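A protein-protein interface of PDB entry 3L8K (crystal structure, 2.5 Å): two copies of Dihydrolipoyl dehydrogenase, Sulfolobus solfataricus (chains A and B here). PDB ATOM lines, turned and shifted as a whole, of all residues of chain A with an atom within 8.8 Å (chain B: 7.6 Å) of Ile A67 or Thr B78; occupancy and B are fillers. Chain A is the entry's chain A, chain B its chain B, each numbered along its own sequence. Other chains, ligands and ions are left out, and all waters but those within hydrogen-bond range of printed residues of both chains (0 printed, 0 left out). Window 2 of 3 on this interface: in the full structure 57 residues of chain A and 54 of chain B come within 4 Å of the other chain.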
ATOM      1  N   GLN A  59       4.035 -10.979 -14.182  1.00  0.00           N
ATOM      2  CA  GLN A  59       3.779 -11.105 -15.606  1.00  0.00           C
ATOM      3  C   GLN A  59       4.118  -9.822 -16.400  1.00  0.00           C
ATOM      4  O   GLN A  59       4.623  -9.907 -17.507  1.00  0.00           O
ATOM      5  CB  GLN A  59       2.327 -11.480 -15.873  1.00  0.00           C
ATOM      6  CG  GLN A  59       2.083 -12.914 -16.214  1.00  0.00           C
ATOM      7  CD  GLN A  59       0.962 -13.091 -17.268  1.00  0.00           C
ATOM      8  OE1 GLN A  59       1.084 -13.920 -18.189  1.00  0.00           O
ATOM      9  NE2 GLN A  59      -0.124 -12.303 -17.136  1.00  0.00           N
ATOM     10  N   THR A  60       3.815  -8.660 -15.835  1.00  0.00           N
ATOM     11  CA  THR A  60       4.156  -7.395 -16.449  1.00  0.00           C
ATOM     12  C   THR A  60       5.667  -7.201 -16.531  1.00  0.00           C
ATOM     13  O   THR A  60       6.189  -6.814 -17.576  1.00  0.00           O
ATOM     14  CB  THR A  60       3.568  -6.222 -15.666  1.00  0.00           C
ATOM     15  OG1 THR A  60       2.176  -6.399 -15.583  1.00  0.00           O
ATOM     16  CG2 THR A  60       3.854  -4.866 -16.339  1.00  0.00           C
ATOM     17  N   ALA A  61       6.365  -7.452 -15.432  1.00  0.00           N
ATOM     18  CA  ALA A  61       7.837  -7.496 -15.463  1.00  0.00           C
ATOM     19  C   ALA A  61       8.375  -8.409 -16.577  1.00  0.00           C
ATOM     20  O   ALA A  61       9.204  -7.993 -17.346  1.00  0.00           O
ATOM     21  CB  ALA A  61       8.400  -7.926 -14.111  1.00  0.00           C
ATOM     22  N   TRP A  62       7.867  -9.628 -16.678  1.00  0.00           N
ATOM     23  CA  TRP A  62       8.364 -10.594 -17.641  1.00  0.00           C
ATOM     24  C   TRP A  62       8.059 -10.227 -19.092  1.00  0.00           C
ATOM     25  O   TRP A  62       8.901 -10.423 -19.962  1.00  0.00           O
ATOM     26  CB  TRP A  62       7.754 -11.957 -17.329  1.00  0.00           C
ATOM     27  CG  TRP A  62       8.116 -13.085 -18.298  1.00  0.00           C
ATOM     28  CD1 TRP A  62       7.339 -13.594 -19.306  1.00  0.00           C
ATOM     29  CD2 TRP A  62       9.324 -13.848 -18.299  1.00  0.00           C
ATOM     30  NE1 TRP A  62       8.001 -14.619 -19.939  1.00  0.00           N
ATOM     31  CE2 TRP A  62       9.222 -14.794 -19.335  1.00  0.00           C
ATOM     32  CE3 TRP A  62      10.495 -13.814 -17.524  1.00  0.00           C
ATOM     33  CZ2 TRP A  62      10.258 -15.704 -19.628  1.00  0.00           C
ATOM     34  CZ3 TRP A  62      11.543 -14.733 -17.811  1.00  0.00           C
ATOM     35  CH2 TRP A  62      11.409 -15.657 -18.853  1.00  0.00           C
ATOM     36  N   ARG A  63       6.853  -9.742 -19.374  1.00  0.00           N
ATOM     37  CA  ARG A  63       6.529  -9.271 -20.731  1.00  0.00           C
ATOM     38  C   ARG A  63       7.457  -8.171 -21.175  1.00  0.00           C
ATOM     39  O   ARG A  63       7.942  -8.174 -22.262  1.00  0.00           O
ATOM     40  CB  ARG A  63       5.087  -8.785 -20.825  1.00  0.00           C
ATOM     41  CG  ARG A  63       4.121  -9.940 -20.758  1.00  0.00           C
ATOM     42  CD  ARG A  63       2.712  -9.521 -20.609  1.00  0.00           C
ATOM     43  NE  ARG A  63       1.889 -10.703 -20.449  1.00  0.00           N
ATOM     44  CZ  ARG A  63       0.572 -10.675 -20.313  1.00  0.00           C
ATOM     45  NH1 ARG A  63      -0.074  -9.522 -20.331  1.00  0.00           N
ATOM     46  NH2 ARG A  63      -0.096 -11.805 -20.163  1.00  0.00           N
ATOM     47  N   LEU A  64       7.714  -7.229 -20.295  1.00  0.00           N
ATOM     48  CA  LEU A  64       8.631  -6.172 -20.595  1.00  0.00           C
ATOM     49  C   LEU A  64      10.040  -6.695 -20.826  1.00  0.00           C
ATOM     50  O   LEU A  64      10.792  -6.133 -21.613  1.00  0.00           O
ATOM     51  CB  LEU A  64       8.635  -5.161 -19.467  1.00  0.00           C
ATOM     52  CG  LEU A  64       9.235  -3.860 -19.949  1.00  0.00           C
ATOM     53  CD1 LEU A  64       8.306  -3.241 -21.029  1.00  0.00           C
ATOM     54  CD2 LEU A  64       9.517  -2.882 -18.777  1.00  0.00           C
ATOM     55  N   THR A  65      10.400  -7.764 -20.128  1.00  0.00           N
ATOM     56  CA  THR A  65      11.702  -8.377 -20.324  1.00  0.00           C
ATOM     57  C   THR A  65      11.801  -9.068 -21.691  1.00  0.00           C
ATOM     58  O   THR A  65      12.841  -9.053 -22.295  1.00  0.00           O
ATOM     59  CB  THR A  65      12.047  -9.318 -19.151  1.00  0.00           C
ATOM     60  OG1 THR A  65      12.164  -8.521 -17.970  1.00  0.00           O
ATOM     61  CG2 THR A  65      13.375 -10.019 -19.362  1.00  0.00           C
ATOM     62  N   ASN A  66      10.712  -9.647 -22.176  1.00  0.00           N
ATOM     63  CA  ASN A  66      10.671 -10.193 -23.533  1.00  0.00           C
ATOM     64  C   ASN A  66      10.627  -9.150 -24.641  1.00  0.00           C
ATOM     65  O   ASN A  66      10.911  -9.467 -25.793  1.00  0.00           O
ATOM     66  CB  ASN A  66       9.461 -11.113 -23.702  1.00  0.00           C
ATOM     67  CG  ASN A  66       9.720 -12.472 -23.187  1.00  0.00           C
ATOM     68  OD1 ASN A  66      10.859 -12.923 -23.240  1.00  0.00           O
ATOM     69  ND2 ASN A  66       8.683 -13.140 -22.636  1.00  0.00           N
ATOM     70  N   ILE A  67      10.248  -7.922 -24.305  1.00  0.00           N
ATOM     71  CA  ILE A  67      10.142  -6.863 -25.292  1.00  0.00           C
ATOM     72  C   ILE A  67      11.412  -6.008 -25.364  1.00  0.00           C
ATOM     73  O   ILE A  67      11.914  -5.753 -26.459  1.00  0.00           O
ATOM     74  CB  ILE A  67       8.941  -5.979 -25.013  1.00  0.00           C
ATOM     75  CG1 ILE A  67       7.653  -6.766 -25.293  1.00  0.00           C
ATOM     76  CG2 ILE A  67       9.029  -4.732 -25.859  1.00  0.00           C
ATOM     77  CD1 ILE A  67       6.458  -6.374 -24.414  1.00  0.00           C
ATOM     78  N   ALA A  68      11.929  -5.569 -24.222  1.00  0.00           N
ATOM     79  CA  ALA A  68      13.143  -4.751 -24.188  1.00  0.00           C
ATOM     80  C   ALA A  68      14.400  -5.633 -24.213  1.00  0.00           C
ATOM     81  O   ALA A  68      15.541  -5.129 -24.245  1.00  0.00           O
ATOM     82  CB  ALA A  68      13.154  -3.872 -22.963  1.00  0.00           C
ATOM     83  N   ASN A  69      14.187  -6.949 -24.183  1.00  0.00           N
ATOM     84  CA  ASN A  69      15.274  -7.932 -24.158  1.00  0.00           C
ATOM     85  C   ASN A  69      16.558  -7.440 -23.461  1.00  0.00           C
ATOM     86  O   ASN A  69      17.649  -7.515 -24.011  1.00  0.00           O
ATOM     87  CB  ASN A  69      15.543  -8.516 -25.569  1.00  0.00           C
ATOM     88  CG  ASN A  69      15.925 -10.018 -25.527  1.00  0.00           C
ATOM     89  OD1 ASN A  69      15.198 -10.842 -24.960  1.00  0.00           O
ATOM     90  ND2 ASN A  69      17.061 -10.365 -26.132  1.00  0.00           N
ATOM     91  N   VAL A  70      16.368  -6.876 -22.266  1.00  0.00           N
ATOM     92  CA  VAL A  70      17.378  -6.800 -21.216  1.00  0.00           C
ATOM     93  C   VAL A  70      16.607  -7.222 -19.961  1.00  0.00           C
ATOM     94  O   VAL A  70      15.377  -7.173 -19.974  1.00  0.00           O
ATOM     95  CB  VAL A  70      17.935  -5.379 -21.046  1.00  0.00           C
ATOM     96  N   SER A 384      -1.671 -10.534 -29.735  1.00  0.00           N
ATOM     97  CA  SER A 384      -1.164 -10.234 -28.381  1.00  0.00           C
ATOM     98  C   SER A 384      -0.157 -11.283 -27.909  1.00  0.00           C
ATOM     99  O   SER A 384       0.867 -10.955 -27.303  1.00  0.00           O
ATOM    100  CB  SER A 384      -2.320 -10.205 -27.379  1.00  0.00           C
ATOM    101  OG  SER A 384      -3.234  -9.170 -27.676  1.00  0.00           O
ATOM    102  N   ALA A 385      -0.439 -12.547 -28.195  1.00  0.00           N
ATOM    103  CA  ALA A 385       0.552 -13.580 -27.946  1.00  0.00           C
ATOM    104  C   ALA A 385       1.909 -13.219 -28.576  1.00  0.00           C
ATOM    105  O   ALA A 385       2.973 -13.434 -27.980  1.00  0.00           O
ATOM    106  CB  ALA A 385       0.052 -14.914 -28.504  1.00  0.00           C
ATOM    107  N   GLN A 386       1.853 -12.679 -29.796  1.00  0.00           N
ATOM    108  CA  GLN A 386       3.051 -12.414 -30.582  1.00  0.00           C
ATOM    109  C   GLN A 386       3.771 -11.194 -30.026  1.00  0.00           C
ATOM    110  O   GLN A 386       4.958 -11.202 -29.894  1.00  0.00           O
ATOM    111  CB  GLN A 386       2.710 -12.288 -32.078  1.00  0.00           C
ATOM    112  CG  GLN A 386       2.045 -13.561 -32.624  1.00  0.00           C
ATOM    113  CD  GLN A 386       1.565 -13.490 -34.072  1.00  0.00           C
ATOM    114  OE1 GLN A 386       1.263 -12.418 -34.578  1.00  0.00           O
ATOM    115  NE2 GLN A 386       1.464 -14.640 -34.723  1.00  0.00           N
ATOM    116  N   ILE A 387       3.028 -10.175 -29.641  1.00  0.00           N
ATOM    117  CA  ILE A 387       3.602  -8.958 -29.100  1.00  0.00           C
ATOM    118  C   ILE A 387       4.401  -9.250 -27.853  1.00  0.00           C
ATOM    119  O   ILE A 387       5.559  -8.777 -27.683  1.00  0.00           O
ATOM    120  CB  ILE A 387       2.513  -7.948 -28.686  1.00  0.00           C
ATOM    121  CG1 ILE A 387       1.750  -7.475 -29.936  1.00  0.00           C
ATOM    122  CG2 ILE A 387       3.185  -6.834 -27.900  1.00  0.00           C
ATOM    123  CD1 ILE A 387       0.461  -6.766 -29.747  1.00  0.00           C
ATOM    124  N   TYR A 388       3.765 -10.020 -26.967  1.00  0.00           N
ATOM    125  CA  TYR A 388       4.352 -10.326 -25.679  1.00  0.00           C
ATOM    126  C   TYR A 388       5.317 -11.497 -25.678  1.00  0.00           C
ATOM    127  O   TYR A 388       5.913 -11.773 -24.653  1.00  0.00           O
ATOM    128  CB  TYR A 388       3.274 -10.686 -24.686  1.00  0.00           C
ATOM    129  CG  TYR A 388       2.259  -9.653 -24.346  1.00  0.00           C
ATOM    130  CD1 TYR A 388       2.591  -8.307 -24.211  1.00  0.00           C
ATOM    131  CD2 TYR A 388       0.953 -10.057 -24.045  1.00  0.00           C
ATOM    132  CE1 TYR A 388       1.614  -7.365 -23.827  1.00  0.00           C
ATOM    133  CE2 TYR A 388      -0.018  -9.152 -23.661  1.00  0.00           C
ATOM    134  CZ  TYR A 388       0.304  -7.810 -23.549  1.00  0.00           C
ATOM    135  OH  TYR A 388      -0.707  -6.946 -23.169  1.00  0.00           O
ATOM    136  N   GLY A 389       5.453 -12.214 -26.780  1.00  0.00           N
ATOM    137  CA  GLY A 389       6.365 -13.354 -26.816  1.00  0.00           C
ATOM    138  C   GLY A 389       5.863 -14.542 -26.003  1.00  0.00           C
ATOM    139  O   GLY A 389       6.643 -15.329 -25.530  1.00  0.00           O
ATOM    140  N   GLN A 390       4.554 -14.692 -25.839  1.00  0.00           N
ATOM    141  CA  GLN A 390       4.006 -15.779 -25.040  1.00  0.00           C
ATOM    142  C   GLN A 390       3.147 -16.595 -25.945  1.00  0.00           C
ATOM    143  O   GLN A 390       1.931 -16.441 -25.950  1.00  0.00           O
ATOM    144  CB  GLN A 390       3.179 -15.219 -23.893  1.00  0.00           C
ATOM    145  CG  GLN A 390       4.002 -14.450 -22.912  1.00  0.00           C
ATOM    146  CD  GLN A 390       3.202 -13.940 -21.748  1.00  0.00           C
ATOM    147  OE1 GLN A 390       2.352 -13.029 -21.885  1.00  0.00           O
ATOM    148  NE2 GLN A 390       3.506 -14.481 -20.560  1.00  0.00           N
ATOM    149  N   THR B  53       0.285  -2.716 -31.250  1.00  0.00           N
ATOM    150  CA  THR B  53       1.575  -3.187 -30.742  1.00  0.00           C
ATOM    151  C   THR B  53       2.356  -2.087 -29.998  1.00  0.00           C
ATOM    152  O   THR B  53       2.884  -2.326 -28.915  1.00  0.00           O
ATOM    153  CB  THR B  53       2.432  -3.768 -31.858  1.00  0.00           C
ATOM    154  OG1 THR B  53       1.709  -4.828 -32.465  1.00  0.00           O
ATOM    155  CG2 THR B  53       3.736  -4.288 -31.355  1.00  0.00           C
ATOM    156  N   GLU B  56       0.504  -1.455 -26.773  1.00  0.00           N
ATOM    157  CA  GLU B  56       0.633  -2.447 -25.711  1.00  0.00           C
ATOM    158  C   GLU B  56       1.998  -2.377 -25.069  1.00  0.00           C
ATOM    159  O   GLU B  56       2.128  -2.428 -23.849  1.00  0.00           O
ATOM    160  CB  GLU B  56       0.312  -3.882 -26.193  1.00  0.00           C
ATOM    161  N   VAL B  57       3.024  -2.218 -25.878  1.00  0.00           N
ATOM    162  CA  VAL B  57       4.380  -2.112 -25.348  1.00  0.00           C
ATOM    163  C   VAL B  57       4.534  -0.925 -24.412  1.00  0.00           C
ATOM    164  O   VAL B  57       5.102  -1.052 -23.360  1.00  0.00           O
ATOM    165  CB  VAL B  57       5.375  -1.904 -26.469  1.00  0.00           C
ATOM    166  CG1 VAL B  57       6.778  -1.618 -25.893  1.00  0.00           C
ATOM    167  CG2 VAL B  57       5.370  -3.091 -27.369  1.00  0.00           C
ATOM    168  N   ILE B  58       4.080   0.256 -24.819  1.00  0.00           N
ATOM    169  CA  ILE B  58       4.326   1.403 -23.991  1.00  0.00           C
ATOM    170  C   ILE B  58       3.402   1.396 -22.756  1.00  0.00           C
ATOM    171  O   ILE B  58       3.790   1.885 -21.700  1.00  0.00           O
ATOM    172  CB  ILE B  58       4.281   2.773 -24.770  1.00  0.00           C
ATOM    173  CG1 ILE B  58       2.874   3.249 -24.930  1.00  0.00           C
ATOM    174  CG2 ILE B  58       5.062   2.746 -26.120  1.00  0.00           C
ATOM    175  CD1 ILE B  58       2.374   3.817 -23.648  1.00  0.00           C
ATOM    176  N   THR B  60       2.571  -1.351 -21.135  1.00  0.00           N
ATOM    177  CA  THR B  60       3.232  -2.281 -20.243  1.00  0.00           C
ATOM    178  C   THR B  60       4.389  -1.579 -19.516  1.00  0.00           C
ATOM    179  O   THR B  60       4.557  -1.739 -18.299  1.00  0.00           O
ATOM    180  CB  THR B  60       3.682  -3.533 -21.014  1.00  0.00           C
ATOM    181  OG1 THR B  60       2.514  -4.174 -21.512  1.00  0.00           O
ATOM    182  CG2 THR B  60       4.422  -4.538 -20.124  1.00  0.00           C
ATOM    183  N   ALA B  61       5.155  -0.747 -20.226  1.00  0.00           N
ATOM    184  CA  ALA B  61       6.237  -0.019 -19.574  1.00  0.00           C
ATOM    185  C   ALA B  61       5.668   0.866 -18.482  1.00  0.00           C
ATOM    186  O   ALA B  61       6.191   0.931 -17.372  1.00  0.00           O
ATOM    187  CB  ALA B  61       7.028   0.798 -20.559  1.00  0.00           C
ATOM    188  N   PRO B  73      14.003   2.257 -18.483  1.00  0.00           N
ATOM    189  CA  PRO B  73      13.850   2.983 -19.746  1.00  0.00           C
ATOM    190  C   PRO B  73      13.999   2.123 -21.037  1.00  0.00           C
ATOM    191  O   PRO B  73      14.932   1.293 -21.178  1.00  0.00           O
ATOM    192  CB  PRO B  73      15.056   3.937 -19.718  1.00  0.00           C
ATOM    193  CG  PRO B  73      16.209   2.961 -19.261  1.00  0.00           C
ATOM    194  CD  PRO B  73      15.441   1.970 -18.250  1.00  0.00           C
ATOM    195  N   LEU B  74      13.125   2.441 -21.996  1.00  0.00           N
ATOM    196  CA  LEU B  74      13.018   1.791 -23.288  1.00  0.00           C
ATOM    197  C   LEU B  74      13.182   2.926 -24.269  1.00  0.00           C
ATOM    198  O   LEU B  74      12.507   3.955 -24.103  1.00  0.00           O
ATOM    199  CB  LEU B  74      11.580   1.303 -23.396  1.00  0.00           C
ATOM    200  CG  LEU B  74      11.220  -0.131 -23.715  1.00  0.00           C
ATOM    201  CD1 LEU B  74       9.677  -0.169 -23.546  1.00  0.00           C
ATOM    202  CD2 LEU B  74      11.631  -0.475 -25.126  1.00  0.00           C
ATOM    203  N   ASP B  75      14.055   2.781 -25.258  1.00  0.00           N
ATOM    204  CA  ASP B  75      14.133   3.762 -26.314  1.00  0.00           C
ATOM    205  C   ASP B  75      12.990   3.491 -27.282  1.00  0.00           C
ATOM    206  O   ASP B  75      12.576   2.336 -27.487  1.00  0.00           O
ATOM    207  CB  ASP B  75      15.469   3.683 -27.047  1.00  0.00           C
ATOM    208  N   PHE B  76      12.478   4.550 -27.888  1.00  0.00           N
ATOM    209  CA  PHE B  76      11.422   4.420 -28.859  1.00  0.00           C
ATOM    210  C   PHE B  76      11.829   3.508 -30.024  1.00  0.00           C
ATOM    211  O   PHE B  76      10.979   2.810 -30.607  1.00  0.00           O
ATOM    212  CB  PHE B  76      10.993   5.790 -29.353  1.00  0.00           C
ATOM    213  CG  PHE B  76       9.876   5.750 -30.342  1.00  0.00           C
ATOM    214  CD1 PHE B  76       8.650   5.225 -29.993  1.00  0.00           C
ATOM    215  CD2 PHE B  76      10.051   6.238 -31.629  1.00  0.00           C
ATOM    216  CE1 PHE B  76       7.629   5.187 -30.876  1.00  0.00           C
ATOM    217  CE2 PHE B  76       9.019   6.209 -32.519  1.00  0.00           C
ATOM    218  CZ  PHE B  76       7.808   5.676 -32.153  1.00  0.00           C
ATOM    219  N   SER B  77      13.121   3.478 -30.350  1.00  0.00           N
ATOM    220  CA  SER B  77      13.570   2.634 -31.451  1.00  0.00           C
ATOM    221  C   SER B  77      13.354   1.155 -31.149  1.00  0.00           C
ATOM    222  O   SER B  77      13.099   0.381 -32.050  1.00  0.00           O
ATOM    223  CB  SER B  77      15.040   2.909 -31.830  1.00  0.00           C
ATOM    224  OG  SER B  77      15.928   2.613 -30.766  1.00  0.00           O
ATOM    225  N   THR B  78      13.449   0.765 -29.889  1.00  0.00           N
ATOM    226  CA  THR B  78      13.182  -0.618 -29.491  1.00  0.00           C
ATOM    227  C   THR B  78      11.684  -0.998 -29.649  1.00  0.00           C
ATOM    228  O   THR B  78      11.359  -2.051 -30.145  1.00  0.00           O
ATOM    229  CB  THR B  78      13.705  -0.842 -28.047  1.00  0.00           C
ATOM    230  OG1 THR B  78      15.147  -0.776 -28.065  1.00  0.00           O
ATOM    231  CG2 THR B  78      13.277  -2.177 -27.484  1.00  0.00           C
ATOM    232  N   VAL B  79      10.795  -0.114 -29.214  1.00  0.00           N
ATOM    233  CA  VAL B  79       9.371  -0.227 -29.451  1.00  0.00           C
ATOM    234  C   VAL B  79       9.094  -0.442 -30.935  1.00  0.00           C
ATOM    235  O   VAL B  79       8.393  -1.387 -31.332  1.00  0.00           O
ATOM    236  CB  VAL B  79       8.662   1.078 -29.035  1.00  0.00           C
ATOM    237  CG1 VAL B  79       7.161   1.020 -29.355  1.00  0.00           C
ATOM    238  CG2 VAL B  79       8.987   1.449 -27.562  1.00  0.00           C
ATOM    239  N   GLN B  80       9.674   0.418 -31.761  1.00  0.00           N
ATOM    240  CA  GLN B  80       9.454   0.340 -33.204  1.00  0.00           C
ATOM    241  C   GLN B  80      10.058  -0.912 -33.795  1.00  0.00           C
ATOM    242  O   GLN B  80       9.590  -1.372 -34.824  1.00  0.00           O
ATOM    243  CB  GLN B  80      10.004   1.576 -33.945  1.00  0.00           C
ATOM    244  CG  GLN B  80       9.299   2.894 -33.643  1.00  0.00           C
ATOM    245  CD  GLN B  80       7.901   2.960 -34.208  1.00  0.00           C
ATOM    246  OE1 GLN B  80       7.010   2.186 -33.807  1.00  0.00           O
ATOM    247  NE2 GLN B  80       7.697   3.873 -35.159  1.00  0.00           N
ATOM    248  N   ASP B  81      11.115  -1.434 -33.188  1.00  0.00           N
ATOM    249  CA  ASP B  81      11.651  -2.764 -33.582  1.00  0.00           C
ATOM    250  C   ASP B  81      10.645  -3.879 -33.251  1.00  0.00           C
ATOM    251  O   ASP B  81      10.513  -4.827 -33.994  1.00  0.00           O
ATOM    252  CB  ASP B  81      12.985  -3.094 -32.898  1.00  0.00           C
ATOM    253  CG  ASP B  81      14.161  -2.260 -33.436  1.00  0.00           C
ATOM    254  OD1 ASP B  81      14.093  -1.750 -34.598  1.00  0.00           O
ATOM    255  OD2 ASP B  81      15.174  -2.132 -32.683  1.00  0.00           O
ATOM    256  N   ARG B  82       9.956  -3.745 -32.124  1.00  0.00           N
ATOM    257  CA  ARG B  82       8.982  -4.706 -31.725  1.00  0.00           C
ATOM    258  C   ARG B  82       7.793  -4.663 -32.659  1.00  0.00           C
ATOM    259  O   ARG B  82       7.238  -5.705 -33.009  1.00  0.00           O
ATOM    260  CB  ARG B  82       8.532  -4.443 -30.309  1.00  0.00           C
ATOM    261  CG  ARG B  82       7.673  -5.568 -29.784  1.00  0.00           C
ATOM    262  CD  ARG B  82       8.462  -6.834 -29.857  1.00  0.00           C
ATOM    263  NE  ARG B  82       7.922  -7.899 -29.050  1.00  0.00           N
ATOM    264  CZ  ARG B  82       8.594  -8.991 -28.728  1.00  0.00           C
ATOM    265  NH1 ARG B  82       9.848  -9.134 -29.122  1.00  0.00           N
ATOM    266  NH2 ARG B  82       8.003  -9.948 -28.001  1.00  0.00           N
ATOM    267  N   LYS B  83       7.430  -3.449 -33.088  1.00  0.00           N
ATOM    268  CA  LYS B  83       6.321  -3.259 -33.999  1.00  0.00           C
ATOM    269  C   LYS B  83       6.667  -3.920 -35.312  1.00  0.00           C
ATOM    270  O   LYS B  83       5.859  -4.655 -35.872  1.00  0.00           O
ATOM    271  CB  LYS B  83       6.042  -1.780 -34.190  1.00  0.00           C
ATOM    272  CG  LYS B  83       4.992  -1.407 -35.242  1.00  0.00           C
ATOM    273  CD  LYS B  83       5.126   0.066 -35.613  1.00  0.00           C
ATOM    274  CE  LYS B  83       6.374   0.343 -36.517  1.00  0.00           C
ATOM    275  NZ  LYS B  83       6.065  -0.191 -37.876  1.00  0.00           N
ATOM    276  N   ASP B  84       7.891  -3.713 -35.778  1.00  0.00           N
ATOM    277  CA  ASP B  84       8.333  -4.312 -37.045  1.00  0.00           C
ATOM    278  C   ASP B  84       8.417  -5.852 -37.012  1.00  0.00           C
ATOM    279  O   ASP B  84       8.108  -6.503 -37.997  1.00  0.00           O
ATOM    280  CB  ASP B  84       9.670  -3.708 -37.470  1.00  0.00           C
ATOM    281  CG  ASP B  84       9.538  -2.284 -38.028  1.00  0.00           C
ATOM    282  OD1 ASP B  84       8.402  -1.826 -38.359  1.00  0.00           O
ATOM    283  OD2 ASP B  84      10.588  -1.611 -38.154  1.00  0.00           O
ATOM    284  N   ARG B 169      11.892   6.940 -36.064  1.00  0.00           N
ATOM    285  CA  ARG B 169      12.469   6.077 -35.048  1.00  0.00           C
ATOM    286  C   ARG B 169      12.971   6.870 -33.840  1.00  0.00           C
ATOM    287  O   ARG B 169      13.641   6.321 -32.970  1.00  0.00           O
ATOM    288  CB  ARG B 169      13.607   5.285 -35.696  1.00  0.00           C
ATOM    289  CG  ARG B 169      13.747   3.847 -35.214  1.00  0.00           C
ATOM    290  CD  ARG B 169      14.254   2.931 -36.328  1.00  0.00           C
ATOM    291  NE  ARG B 169      13.137   2.441 -37.129  1.00  0.00           N
ATOM    292  CZ  ARG B 169      12.521   1.278 -36.920  1.00  0.00           C
ATOM    293  NH1 ARG B 169      11.504   0.917 -37.690  1.00  0.00           N
ATOM    294  NH2 ARG B 169      12.931   0.480 -35.941  1.00  0.00           N
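Thr B60 touches Thr A60. Asn A66 touches Arg B82 (O to NH1, 3.5 Å). Val B57 touches Ile A67. Ile A67 touches Thr B78 (O to CG2, 3.96 Å). CG1 of Ile A67 touches NE of Arg B82 (3.9 Å). Gln A386 touches Arg B82 (O to NH2, 3.8 Å). Thr B53 touches Ile A387. Tyr A388 touches Arg B82 (C to NH2, 3.9 Å). Gly A389 touches Arg B82 (N to NH2, 3.6 Å).
The backbone carbonyl oxygen of Ile A387 sits at hydrogen-bond distance from the guanidinium group of Arg B82 (2.7 Å).
Thr B78 touches one residue of chain A. Of the printed residues of chain A, Val B57 touches Ile A67. Printed residues of chain B within 4 Å of Asn A66: Arg B82 (3.5 Å). Printed residues of chain B within 4 Å of Tyr A388: Arg B82 (3.9 Å). Printed residues of chain A within 4 Å of Thr B53: Ile A387. Val B79 touches none of the printed residues of chain A. Phe B76 touches none of the printed residues of chain A. The nearest residue of chain A that does not touch Thr B78 is Ala A68 (4.2 Å).
Of the 19 printed residues of chain A, 7 touch a printed residue of chain B. Printed residues of chain A that touch a printed residue of chain B: Thr A60, Asn A66, Ile A67, Gln A386, Ile A387, Tyr A388 and Gly A389. Hydrophobic or aromatic side chains of chain A within 4 Å of the printed part of chain B: Ile A67 and Ile A387. Of the 19 printed residues of chain B, 5 touch a printed residue of chain A. Printed residues of chain B that touch a printed residue of chain A: Thr B53, Val B57, Thr B60, Thr B78 and Arg B82. Hydrophobic or aromatic side chains of chain B within 4 Å of the printed part of chain A: Val B57. Among the printed residues, 10 pairs touch across the chains.
Thr A60 touches its own counterpart, Thr B60. 2 positions are printed for both chains. Of the 10 pairs that touch across the chains among the printed residues, 1 has its exchanged pair printed and touching as well.
The indole nitrogen of Trp A62 lies close to the side-chain amide nitrogen of Asn A66, at 3.2 Å. The backbone carbonyl oxygen (O) of Glu B56 is in hydrogen-bond range of the side-chain hydroxyl (OG1) of Thr B60 (2.9 Å).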
